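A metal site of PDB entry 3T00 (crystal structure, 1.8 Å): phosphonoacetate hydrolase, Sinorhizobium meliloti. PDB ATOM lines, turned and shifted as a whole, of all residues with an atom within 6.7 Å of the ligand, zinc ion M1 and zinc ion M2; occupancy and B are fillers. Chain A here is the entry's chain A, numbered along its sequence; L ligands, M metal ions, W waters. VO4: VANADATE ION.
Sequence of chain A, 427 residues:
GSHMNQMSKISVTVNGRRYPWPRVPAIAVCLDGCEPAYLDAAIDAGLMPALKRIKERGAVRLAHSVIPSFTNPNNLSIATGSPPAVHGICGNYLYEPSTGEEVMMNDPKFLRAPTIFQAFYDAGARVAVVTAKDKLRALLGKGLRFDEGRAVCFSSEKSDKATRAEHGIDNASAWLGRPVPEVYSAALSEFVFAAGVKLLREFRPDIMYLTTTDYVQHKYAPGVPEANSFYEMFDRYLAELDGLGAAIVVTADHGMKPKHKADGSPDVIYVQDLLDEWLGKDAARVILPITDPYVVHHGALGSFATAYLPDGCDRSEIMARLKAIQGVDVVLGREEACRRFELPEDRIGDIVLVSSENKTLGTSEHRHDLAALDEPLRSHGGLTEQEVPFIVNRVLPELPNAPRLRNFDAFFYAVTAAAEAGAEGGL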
ATOM      1  N   CYS A  30      25.853 -10.822  21.250  1.00  0.00           N
ATOM      2  CA  CYS A  30      24.746 -11.774  21.357  1.00  0.00           C
ATOM      3  C   CYS A  30      23.983 -11.503  22.638  1.00  0.00           C
ATOM      4  O   CYS A  30      24.476 -11.819  23.729  1.00  0.00           O
ATOM      5  CB  CYS A  30      25.250 -13.212  21.352  1.00  0.00           C
ATOM      6  SG  CYS A  30      23.940 -14.470  21.502  1.00  0.00           S
ATOM      7  N   ASP A  32      21.507 -12.806  24.730  1.00  0.00           N
ATOM      8  CA  ASP A  32      20.901 -14.119  24.949  1.00  0.00           C
ATOM      9  C   ASP A  32      19.409 -14.003  25.246  1.00  0.00           C
ATOM     10  O   ASP A  32      18.987 -13.244  26.123  1.00  0.00           O
ATOM     11  CB  ASP A  32      21.617 -14.796  26.124  1.00  0.00           C
ATOM     12  CG  ASP A  32      21.504 -16.292  26.081  1.00  0.00           C
ATOM     13  OD1 ASP A  32      20.372 -16.799  25.920  1.00  0.00           O
ATOM     14  OD2 ASP A  32      22.558 -16.966  26.206  1.00  0.00           O
ATOM     15  N   GLY A  33      18.596 -14.742  24.489  1.00  0.00           N
ATOM     16  CA  GLY A  33      17.153 -14.803  24.721  1.00  0.00           C
ATOM     17  C   GLY A  33      16.393 -13.514  24.424  1.00  0.00           C
ATOM     18  O   GLY A  33      15.255 -13.343  24.857  1.00  0.00           O
ATOM     19  N   SER A  69      16.340 -23.608  18.625  1.00  0.00           N
ATOM     20  CA  SER A  69      16.653 -22.259  19.101  1.00  0.00           C
ATOM     21  C   SER A  69      17.145 -22.321  20.557  1.00  0.00           C
ATOM     22  O   SER A  69      16.493 -21.825  21.481  1.00  0.00           O
ATOM     23  CB  SER A  69      15.451 -21.313  18.907  1.00  0.00           C
ATOM     24  OG  SER A  69      14.259 -21.804  19.514  1.00  0.00           O
ATOM     25  N   PHE A  70      18.313 -22.948  20.738  1.00  0.00           N
ATOM     26  CA  PHE A  70      18.990 -23.039  22.041  1.00  0.00           C
ATOM     27  C   PHE A  70      20.334 -22.301  21.999  1.00  0.00           C
ATOM     28  O   PHE A  70      20.824 -21.960  20.929  1.00  0.00           O
ATOM     29  CB  PHE A  70      19.246 -24.509  22.434  1.00  0.00           C
ATOM     30  CG  PHE A  70      17.995 -25.312  22.709  1.00  0.00           C
ATOM     31  CD1 PHE A  70      16.954 -24.786  23.473  1.00  0.00           C
ATOM     32  CD2 PHE A  70      17.875 -26.614  22.236  1.00  0.00           C
ATOM     33  CE1 PHE A  70      15.797 -25.525  23.737  1.00  0.00           C
ATOM     34  CE2 PHE A  70      16.725 -27.374  22.503  1.00  0.00           C
ATOM     35  CZ  PHE A  70      15.684 -26.827  23.240  1.00  0.00           C
ATOM     36  N   THR A  71      20.923 -22.090  23.167  1.00  0.00           N
ATOM     37  CA  THR A  71      22.133 -21.275  23.340  1.00  0.00           C
ATOM     38  C   THR A  71      23.363 -21.781  22.612  1.00  0.00           C
ATOM     39  O   THR A  71      23.931 -21.084  21.781  1.00  0.00           O
ATOM     40  CB  THR A  71      22.508 -21.155  24.839  1.00  0.00           C
ATOM     41  OG1 THR A  71      21.366 -20.680  25.551  1.00  0.00           O
ATOM     42  CG2 THR A  71      23.673 -20.192  25.057  1.00  0.00           C
ATOM     43  N   ASN A  72      23.794 -23.001  22.946  1.00  0.00           N
ATOM     44  CA  ASN A  72      25.003 -23.555  22.362  1.00  0.00           C
ATOM     45  C   ASN A  72      24.981 -23.704  20.842  1.00  0.00           C
ATOM     46  O   ASN A  72      25.916 -23.242  20.183  1.00  0.00           O
ATOM     47  CB  ASN A  72      25.440 -24.839  23.086  1.00  0.00           C
ATOM     48  CG  ASN A  72      26.088 -24.545  24.428  1.00  0.00           C
ATOM     49  OD1 ASN A  72      26.015 -23.417  24.925  1.00  0.00           O
ATOM     50  ND2 ASN A  72      26.739 -25.547  25.001  1.00  0.00           N
ATOM     51  N   PRO A  73      23.915 -24.317  20.258  1.00  0.00           N
ATOM     52  CA  PRO A  73      23.935 -24.434  18.785  1.00  0.00           C
ATOM     53  C   PRO A  73      24.002 -23.077  18.103  1.00  0.00           C
ATOM     54  O   PRO A  73      24.716 -22.910  17.106  1.00  0.00           O
ATOM     55  CB  PRO A  73      22.615 -25.132  18.462  1.00  0.00           C
ATOM     56  CG  PRO A  73      22.224 -25.814  19.740  1.00  0.00           C
ATOM     57  CD  PRO A  73      22.728 -24.971  20.855  1.00  0.00           C
ATOM     58  N   ASN A  75      25.094 -19.972  19.488  1.00  0.00           N
ATOM     59  CA  ASN A  75      26.375 -19.312  19.748  1.00  0.00           C
ATOM     60  C   ASN A  75      27.487 -19.892  18.874  1.00  0.00           C
ATOM     61  O   ASN A  75      28.304 -19.163  18.323  1.00  0.00           O
ATOM     62  CB  ASN A  75      26.739 -19.381  21.237  1.00  0.00           C
ATOM     63  CG  ASN A  75      26.121 -18.250  22.026  1.00  0.00           C
ATOM     64  OD1 ASN A  75      25.008 -18.378  22.551  1.00  0.00           O
ATOM     65  ND2 ASN A  75      26.828 -17.136  22.107  1.00  0.00           N
ATOM     66  N   ASN A  92      23.130 -29.836  23.996  1.00  0.00           N
ATOM     67  CA  ASN A  92      24.033 -29.794  25.153  1.00  0.00           C
ATOM     68  C   ASN A  92      24.632 -31.150  25.504  1.00  0.00           C
ATOM     69  O   ASN A  92      25.619 -31.225  26.240  1.00  0.00           O
ATOM     70  CB  ASN A  92      23.330 -29.180  26.368  1.00  0.00           C
ATOM     71  CG  ASN A  92      23.350 -27.657  26.340  1.00  0.00           C
ATOM     72  OD1 ASN A  92      23.915 -27.043  25.431  1.00  0.00           O
ATOM     73  ND2 ASN A  92      22.740 -27.047  27.345  1.00  0.00           N
ATOM     74  N   LYS A 135      31.775 -22.590  30.257  1.00  0.00           N
ATOM     75  CA  LYS A 135      31.818 -23.762  29.358  1.00  0.00           C
ATOM     76  C   LYS A 135      31.685 -23.333  27.893  1.00  0.00           C
ATOM     77  O   LYS A 135      32.338 -23.906  27.009  1.00  0.00           O
ATOM     78  CB  LYS A 135      30.847 -24.887  29.777  1.00  0.00           C
ATOM     79  CG  LYS A 135      29.363 -24.644  29.601  1.00  0.00           C
ATOM     80  CD  LYS A 135      28.838 -25.230  28.286  1.00  0.00           C
ATOM     81  CE  LYS A 135      27.443 -25.817  28.426  1.00  0.00           C
ATOM     82  NZ  LYS A 135      26.404 -24.809  28.746  1.00  0.00           N
ATOM     83  N   THR A 212      26.139 -13.308  26.295  1.00  0.00           N
ATOM     84  CA  THR A 212      25.572 -13.123  27.631  1.00  0.00           C
ATOM     85  C   THR A 212      24.783 -14.369  28.059  1.00  0.00           C
ATOM     86  O   THR A 212      24.977 -15.440  27.479  1.00  0.00           O
ATOM     87  CB  THR A 212      24.692 -11.862  27.669  1.00  0.00           C
ATOM     88  OG1 THR A 212      23.675 -11.948  26.661  1.00  0.00           O
ATOM     89  CG2 THR A 212      25.530 -10.625  27.397  1.00  0.00           C
ATOM     90  N   THR A 213      23.922 -14.242  29.085  1.00  0.00           N
ATOM     91  CA  THR A 213      22.957 -15.304  29.445  1.00  0.00           C
ATOM     92  C   THR A 213      21.525 -14.779  29.467  1.00  0.00           C
ATOM     93  O   THR A 213      21.312 -13.572  29.567  1.00  0.00           O
ATOM     94  CB  THR A 213      23.230 -15.989  30.823  1.00  0.00           C
ATOM     95  OG1 THR A 213      22.762 -15.142  31.889  1.00  0.00           O
ATOM     96  CG2 THR A 213      24.704 -16.296  31.013  1.00  0.00           C
ATOM     97  N   ASP A 214      20.559 -15.690  29.381  1.00  0.00           N
ATOM     98  CA  ASP A 214      19.134 -15.314  29.351  1.00  0.00           C
ATOM     99  C   ASP A 214      18.437 -15.480  30.723  1.00  0.00           C
ATOM    100  O   ASP A 214      17.223 -15.704  30.796  1.00  0.00           O
ATOM    101  CB  ASP A 214      18.378 -16.053  28.231  1.00  0.00           C
ATOM    102  CG  ASP A 214      18.366 -17.567  28.419  1.00  0.00           C
ATOM    103  OD1 ASP A 214      19.050 -18.104  29.314  1.00  0.00           O
ATOM    104  OD2 ASP A 214      17.643 -18.240  27.638  1.00  0.00           O
ATOM    105  N   TYR A 215      19.223 -15.342  31.780  1.00  0.00           N
ATOM    106  CA  TYR A 215      18.697 -15.359  33.152  1.00  0.00           C
ATOM    107  C   TYR A 215      17.494 -14.424  33.329  1.00  0.00           C
ATOM    108  O   TYR A 215      16.417 -14.863  33.765  1.00  0.00           O
ATOM    109  CB  TYR A 215      19.796 -15.026  34.170  1.00  0.00           C
ATOM    110  CG  TYR A 215      19.222 -14.837  35.560  1.00  0.00           C
ATOM    111  CD1 TYR A 215      18.819 -15.933  36.322  1.00  0.00           C
ATOM    112  CD2 TYR A 215      19.017 -13.559  36.085  1.00  0.00           C
ATOM    113  CE1 TYR A 215      18.250 -15.777  37.581  1.00  0.00           C
ATOM    114  CE2 TYR A 215      18.454 -13.387  37.346  1.00  0.00           C
ATOM    115  CZ  TYR A 215      18.077 -14.494  38.085  1.00  0.00           C
ATOM    116  OH  TYR A 215      17.523 -14.325  39.337  1.00  0.00           O
ATOM    117  N   HIS A 218      14.329 -15.424  30.998  1.00  0.00           N
ATOM    118  CA  HIS A 218      13.558 -16.587  31.456  1.00  0.00           C
ATOM    119  C   HIS A 218      12.597 -16.204  32.590  1.00  0.00           C
ATOM    120  O   HIS A 218      11.545 -16.835  32.775  1.00  0.00           O
ATOM    121  CB  HIS A 218      14.481 -17.697  31.934  1.00  0.00           C
ATOM    122  CG  HIS A 218      14.918 -18.642  30.845  1.00  0.00           C
ATOM    123  ND1 HIS A 218      14.062 -19.546  30.256  1.00  0.00           N
ATOM    124  CD2 HIS A 218      16.125 -18.815  30.258  1.00  0.00           C
ATOM    125  CE1 HIS A 218      14.728 -20.246  29.351  1.00  0.00           C
ATOM    126  NE2 HIS A 218      15.970 -19.817  29.323  1.00  0.00           N
ATOM    127  N   ASP A 253      20.953 -15.219  20.212  1.00  0.00           N
ATOM    128  CA  ASP A 253      20.974 -16.661  19.915  1.00  0.00           C
ATOM    129  C   ASP A 253      19.595 -17.261  19.633  1.00  0.00           C
ATOM    130  O   ASP A 253      19.456 -18.208  18.857  1.00  0.00           O
ATOM    131  CB  ASP A 253      21.701 -17.451  21.013  1.00  0.00           C
ATOM    132  CG  ASP A 253      21.146 -17.184  22.417  1.00  0.00           C
ATOM    133  OD1 ASP A 253      20.259 -16.307  22.613  1.00  0.00           O
ATOM    134  OD2 ASP A 253      21.650 -17.857  23.331  1.00  0.00           O
ATOM    135  N   HIS A 254      18.576 -16.697  20.288  1.00  0.00           N
ATOM    136  CA  HIS A 254      17.188 -17.144  20.168  1.00  0.00           C
ATOM    137  C   HIS A 254      16.305 -16.143  20.907  1.00  0.00           C
ATOM    138  O   HIS A 254      16.821 -15.303  21.633  1.00  0.00           O
ATOM    139  CB  HIS A 254      17.007 -18.523  20.799  1.00  0.00           C
ATOM    140  CG  HIS A 254      17.504 -18.608  22.214  1.00  0.00           C
ATOM    141  ND1 HIS A 254      16.798 -18.095  23.284  1.00  0.00           N
ATOM    142  CD2 HIS A 254      18.646 -19.121  22.723  1.00  0.00           C
ATOM    143  CE1 HIS A 254      17.490 -18.283  24.387  1.00  0.00           C
ATOM    144  NE2 HIS A 254      18.611 -18.900  24.076  1.00  0.00           N
ATOM    145  N   GLY A 255      15.002 -16.267  20.721  1.00  0.00           N
ATOM    146  CA  GLY A 255      14.021 -15.432  21.406  1.00  0.00           C
ATOM    147  C   GLY A 255      13.540 -16.070  22.695  1.00  0.00           C
ATOM    148  O   GLY A 255      14.236 -16.890  23.306  1.00  0.00           O
ATOM    149  N   MET A 256      12.327 -15.701  23.100  1.00  0.00           N
ATOM    150  CA  MET A 256      11.781 -16.138  24.380  1.00  0.00           C
ATOM    151  C   MET A 256      10.275 -15.955  24.339  1.00  0.00           C
ATOM    152  O   MET A 256       9.789 -14.911  23.927  1.00  0.00           O
ATOM    153  CB  MET A 256      12.394 -15.312  25.528  1.00  0.00           C
ATOM    154  CG  MET A 256      12.105 -15.835  26.938  1.00  0.00           C
ATOM    155  SD  MET A 256      12.911 -17.401  27.354  1.00  0.00           S
ATOM    156  CE  MET A 256      14.610 -16.907  27.567  1.00  0.00           C
ATOM    157  N   PRO A 289      17.602 -31.443  24.387  1.00  0.00           N
ATOM    158  CA  PRO A 289      18.888 -30.788  24.170  1.00  0.00           C
ATOM    159  C   PRO A 289      19.092 -29.446  24.895  1.00  0.00           C
ATOM    160  O   PRO A 289      20.221 -28.952  24.922  1.00  0.00           O
ATOM    161  CB  PRO A 289      18.931 -30.569  22.645  1.00  0.00           C
ATOM    162  CG  PRO A 289      17.864 -31.468  22.094  1.00  0.00           C
ATOM    163  CD  PRO A 289      16.807 -31.503  23.138  1.00  0.00           C
ATOM    164  N   ILE A 290      18.028 -28.880  25.472  1.00  0.00           N
ATOM    165  CA  ILE A 290      18.081 -27.546  26.095  1.00  0.00           C
ATOM    166  C   ILE A 290      19.205 -27.385  27.135  1.00  0.00           C
ATOM    167  O   ILE A 290      19.930 -26.382  27.117  1.00  0.00           O
ATOM    168  CB  ILE A 290      16.712 -27.097  26.691  1.00  0.00           C
ATOM    169  CG1 ILE A 290      16.812 -25.670  27.260  1.00  0.00           C
ATOM    170  CG2 ILE A 290      16.193 -28.086  27.741  1.00  0.00           C
ATOM    171  CD1 ILE A 290      15.482 -24.951  27.426  1.00  0.00           C
ATOM    172  N   THR A 291      19.343 -28.364  28.017  1.00  0.00           N
ATOM    173  CA  THR A 291      20.381 -28.323  29.058  1.00  0.00           C
ATOM    174  C   THR A 291      20.736 -29.718  29.587  1.00  0.00           C
ATOM    175  O   THR A 291      20.055 -30.701  29.277  1.00  0.00           O
ATOM    176  CB  THR A 291      20.016 -27.356  30.215  1.00  0.00           C
ATOM    177  OG1 THR A 291      21.134 -27.217  31.099  1.00  0.00           O
ATOM    178  CG2 THR A 291      18.795 -27.847  30.995  1.00  0.00           C
ATOM    179  N   GLY A 299      14.383 -26.545  34.811  1.00  0.00           N
ATOM    180  CA  GLY A 299      15.259 -25.868  33.860  1.00  0.00           C
ATOM    181  C   GLY A 299      15.467 -26.614  32.564  1.00  0.00           C
ATOM    182  O   GLY A 299      16.088 -26.093  31.630  1.00  0.00           O
ATOM    183  N   ARG A 378       8.886 -19.403  31.157  1.00  0.00           N
ATOM    184  CA  ARG A 378       9.254 -18.792  29.881  1.00  0.00           C
ATOM    185  C   ARG A 378      10.419 -19.601  29.329  1.00  0.00           C
ATOM    186  O   ARG A 378      11.360 -19.923  30.061  1.00  0.00           O
ATOM    187  CB  ARG A 378       9.676 -17.332  30.065  1.00  0.00           C
ATOM    188  CG  ARG A 378       8.583 -16.430  30.630  1.00  0.00           C
ATOM    189  CD  ARG A 378       9.087 -15.006  30.887  1.00  0.00           C
ATOM    190  NE  ARG A 378       9.677 -14.400  29.687  1.00  0.00           N
ATOM    191  CZ  ARG A 378       8.983 -13.968  28.640  1.00  0.00           C
ATOM    192  NH1 ARG A 378       7.662 -14.074  28.607  1.00  0.00           N
ATOM    193  NH2 ARG A 378       9.630 -13.446  27.599  1.00  0.00           N
ATOM    194  N   SER A 379      10.359 -19.933  28.046  1.00  0.00           N
ATOM    195  CA  SER A 379      11.437 -20.719  27.450  1.00  0.00           C
ATOM    196  C   SER A 379      11.544 -20.520  25.945  1.00  0.00           C
ATOM    197  O   SER A 379      10.925 -19.612  25.373  1.00  0.00           O
ATOM    198  CB  SER A 379      11.307 -22.205  27.798  1.00  0.00           C
ATOM    199  OG  SER A 379      12.577 -22.826  27.754  1.00  0.00           O
ATOM    200  N   HIS A 380      12.318 -21.397  25.334  1.00  0.00           N
ATOM    201  CA  HIS A 380      12.651 -21.308  23.911  1.00  0.00           C
ATOM    202  C   HIS A 380      13.012 -22.678  23.362  1.00  0.00           C
ATOM    203  O   HIS A 380      12.850 -23.718  24.051  1.00  0.00           O
ATOM    204  CB  HIS A 380      13.802 -20.307  23.714  1.00  0.00           C
ATOM    205  CG  HIS A 380      14.945 -20.529  24.644  1.00  0.00           C
ATOM    206  ND1 HIS A 380      16.038 -21.311  24.330  1.00  0.00           N
ATOM    207  CD2 HIS A 380      15.160 -20.084  25.917  1.00  0.00           C
ATOM    208  CE1 HIS A 380      16.870 -21.335  25.347  1.00  0.00           C
ATOM    209  NE2 HIS A 380      16.368 -20.590  26.319  1.00  0.00           N
HETATM  210  V   VO4 L   1      20.075 -21.358  26.969  1.00  0.00           V
HETATM  211  O1  VO4 L   1      21.749 -21.506  27.833  1.00  0.00           O
HETATM  212  O2  VO4 L   1      18.730 -21.544  28.316  1.00  0.00           O
HETATM  213  O3  VO4 L   1      19.793 -22.759  25.684  1.00  0.00           O
HETATM  214  O4  VO4 L   1      19.607 -19.625  26.330  1.00  0.00           O
HETATM  215 ZN    ZN M   1      20.507 -18.627  25.128  1.00  0.00          ZN
HETATM  216 ZN    ZN M   2      17.547 -20.031  27.914  1.00  0.00          ZN
HETATM  217  O   HOH W   1      22.103 -18.500  28.325  1.00  0.00           O
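Zinc ion M2 is bound by the side-chain carboxylate of Asp 214, an oxygen (O2) of the ligand, a ring nitrogen (NE2) of His 380 and a ring nitrogen (NE2) of His 218. Zinc ion M2 has four donor atoms within binding distance. Slightly farther from zinc ion M2 lies an oxygen (O4) of the ligand (2.6 Å). Slightly farther from zinc ion M2 lies OD1 of Asp 214 (2.8 Å).
The side-chain hydroxyl (OG1) of Thr 71 is bound to a vanadium atom (V) of the ligand (2.0 Å).
Water W1 lies within hydrogen-bond range of the side-chain carboxylate (OD2) of Asp 32 and the side-chain carboxylate (OD1) of Asp 214.
The backbone NH of Asp 32 is in hydrogen-bond range of the side-chain hydroxyl of Thr 212, 3.0 Å away. O of Thr 71 lies close to OD1 of Asn 75, 3.0 Å away. A ring nitrogen (ND1) of His 380 sits close to a ring nitrogen (ND1) of His 254 (3.5 Å). The backbone carbonyl oxygen (O) of Ser 69 sits at hydrogen-bond distance from a ring nitrogen (ND1) of His 380, at 2.9 Å. ND1 of His 218 lies within hydrogen-bond range of SD of Met 256 (3.8 Å). OD1 of Asp 253 is in hydrogen-bond range of N of Gly 33 (3.0 Å). The side-chain amide oxygen (OD1) of Asn 75 sits close to the side-chain carboxylate (OD2) of Asp 253 (3.5 Å). The backbone NH (N) of Asp 253 is in hydrogen-bond range of the side-chain sulfur (SG) of Cys 30, at 3.3 Å.
Four residues have an atom within 4 Å of zinc ion M2: Asp 214, His 218, His 254 and His 380. The nearest printed residue that does not touch zinc ion M2 is Met 256 (4.3 Å).
Phe 70 touches the ligand (CB to O3, 3.7 Å). O of Ile 290 touches O3 of the ligand (3.9 Å). Hydrophobic or aromatic side chains within 4 Å of the ligand: Phe 70, His 254 and His 380. The nearest printed residue that does not touch the ligand is Asp 253 (4.04 Å).
An oxygen (O4) of the ligand is bound to zinc ion M1 (1.8 Å). OD1 of Asp 32 is bound to zinc ion M1 (2.0 Å). NE2 of His 254 binds zinc ion M1 (2.2 Å). The side-chain carboxylate (OD2) of Asp 253 is bound to zinc ion M1 (2.3 Å). OG1 of Thr 71 binds zinc ion M1, at 2.3 Å.
Within 4 Å of zinc ion M1: Asp 32, Thr 71, Asp 214, Asp 253 and His 254.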
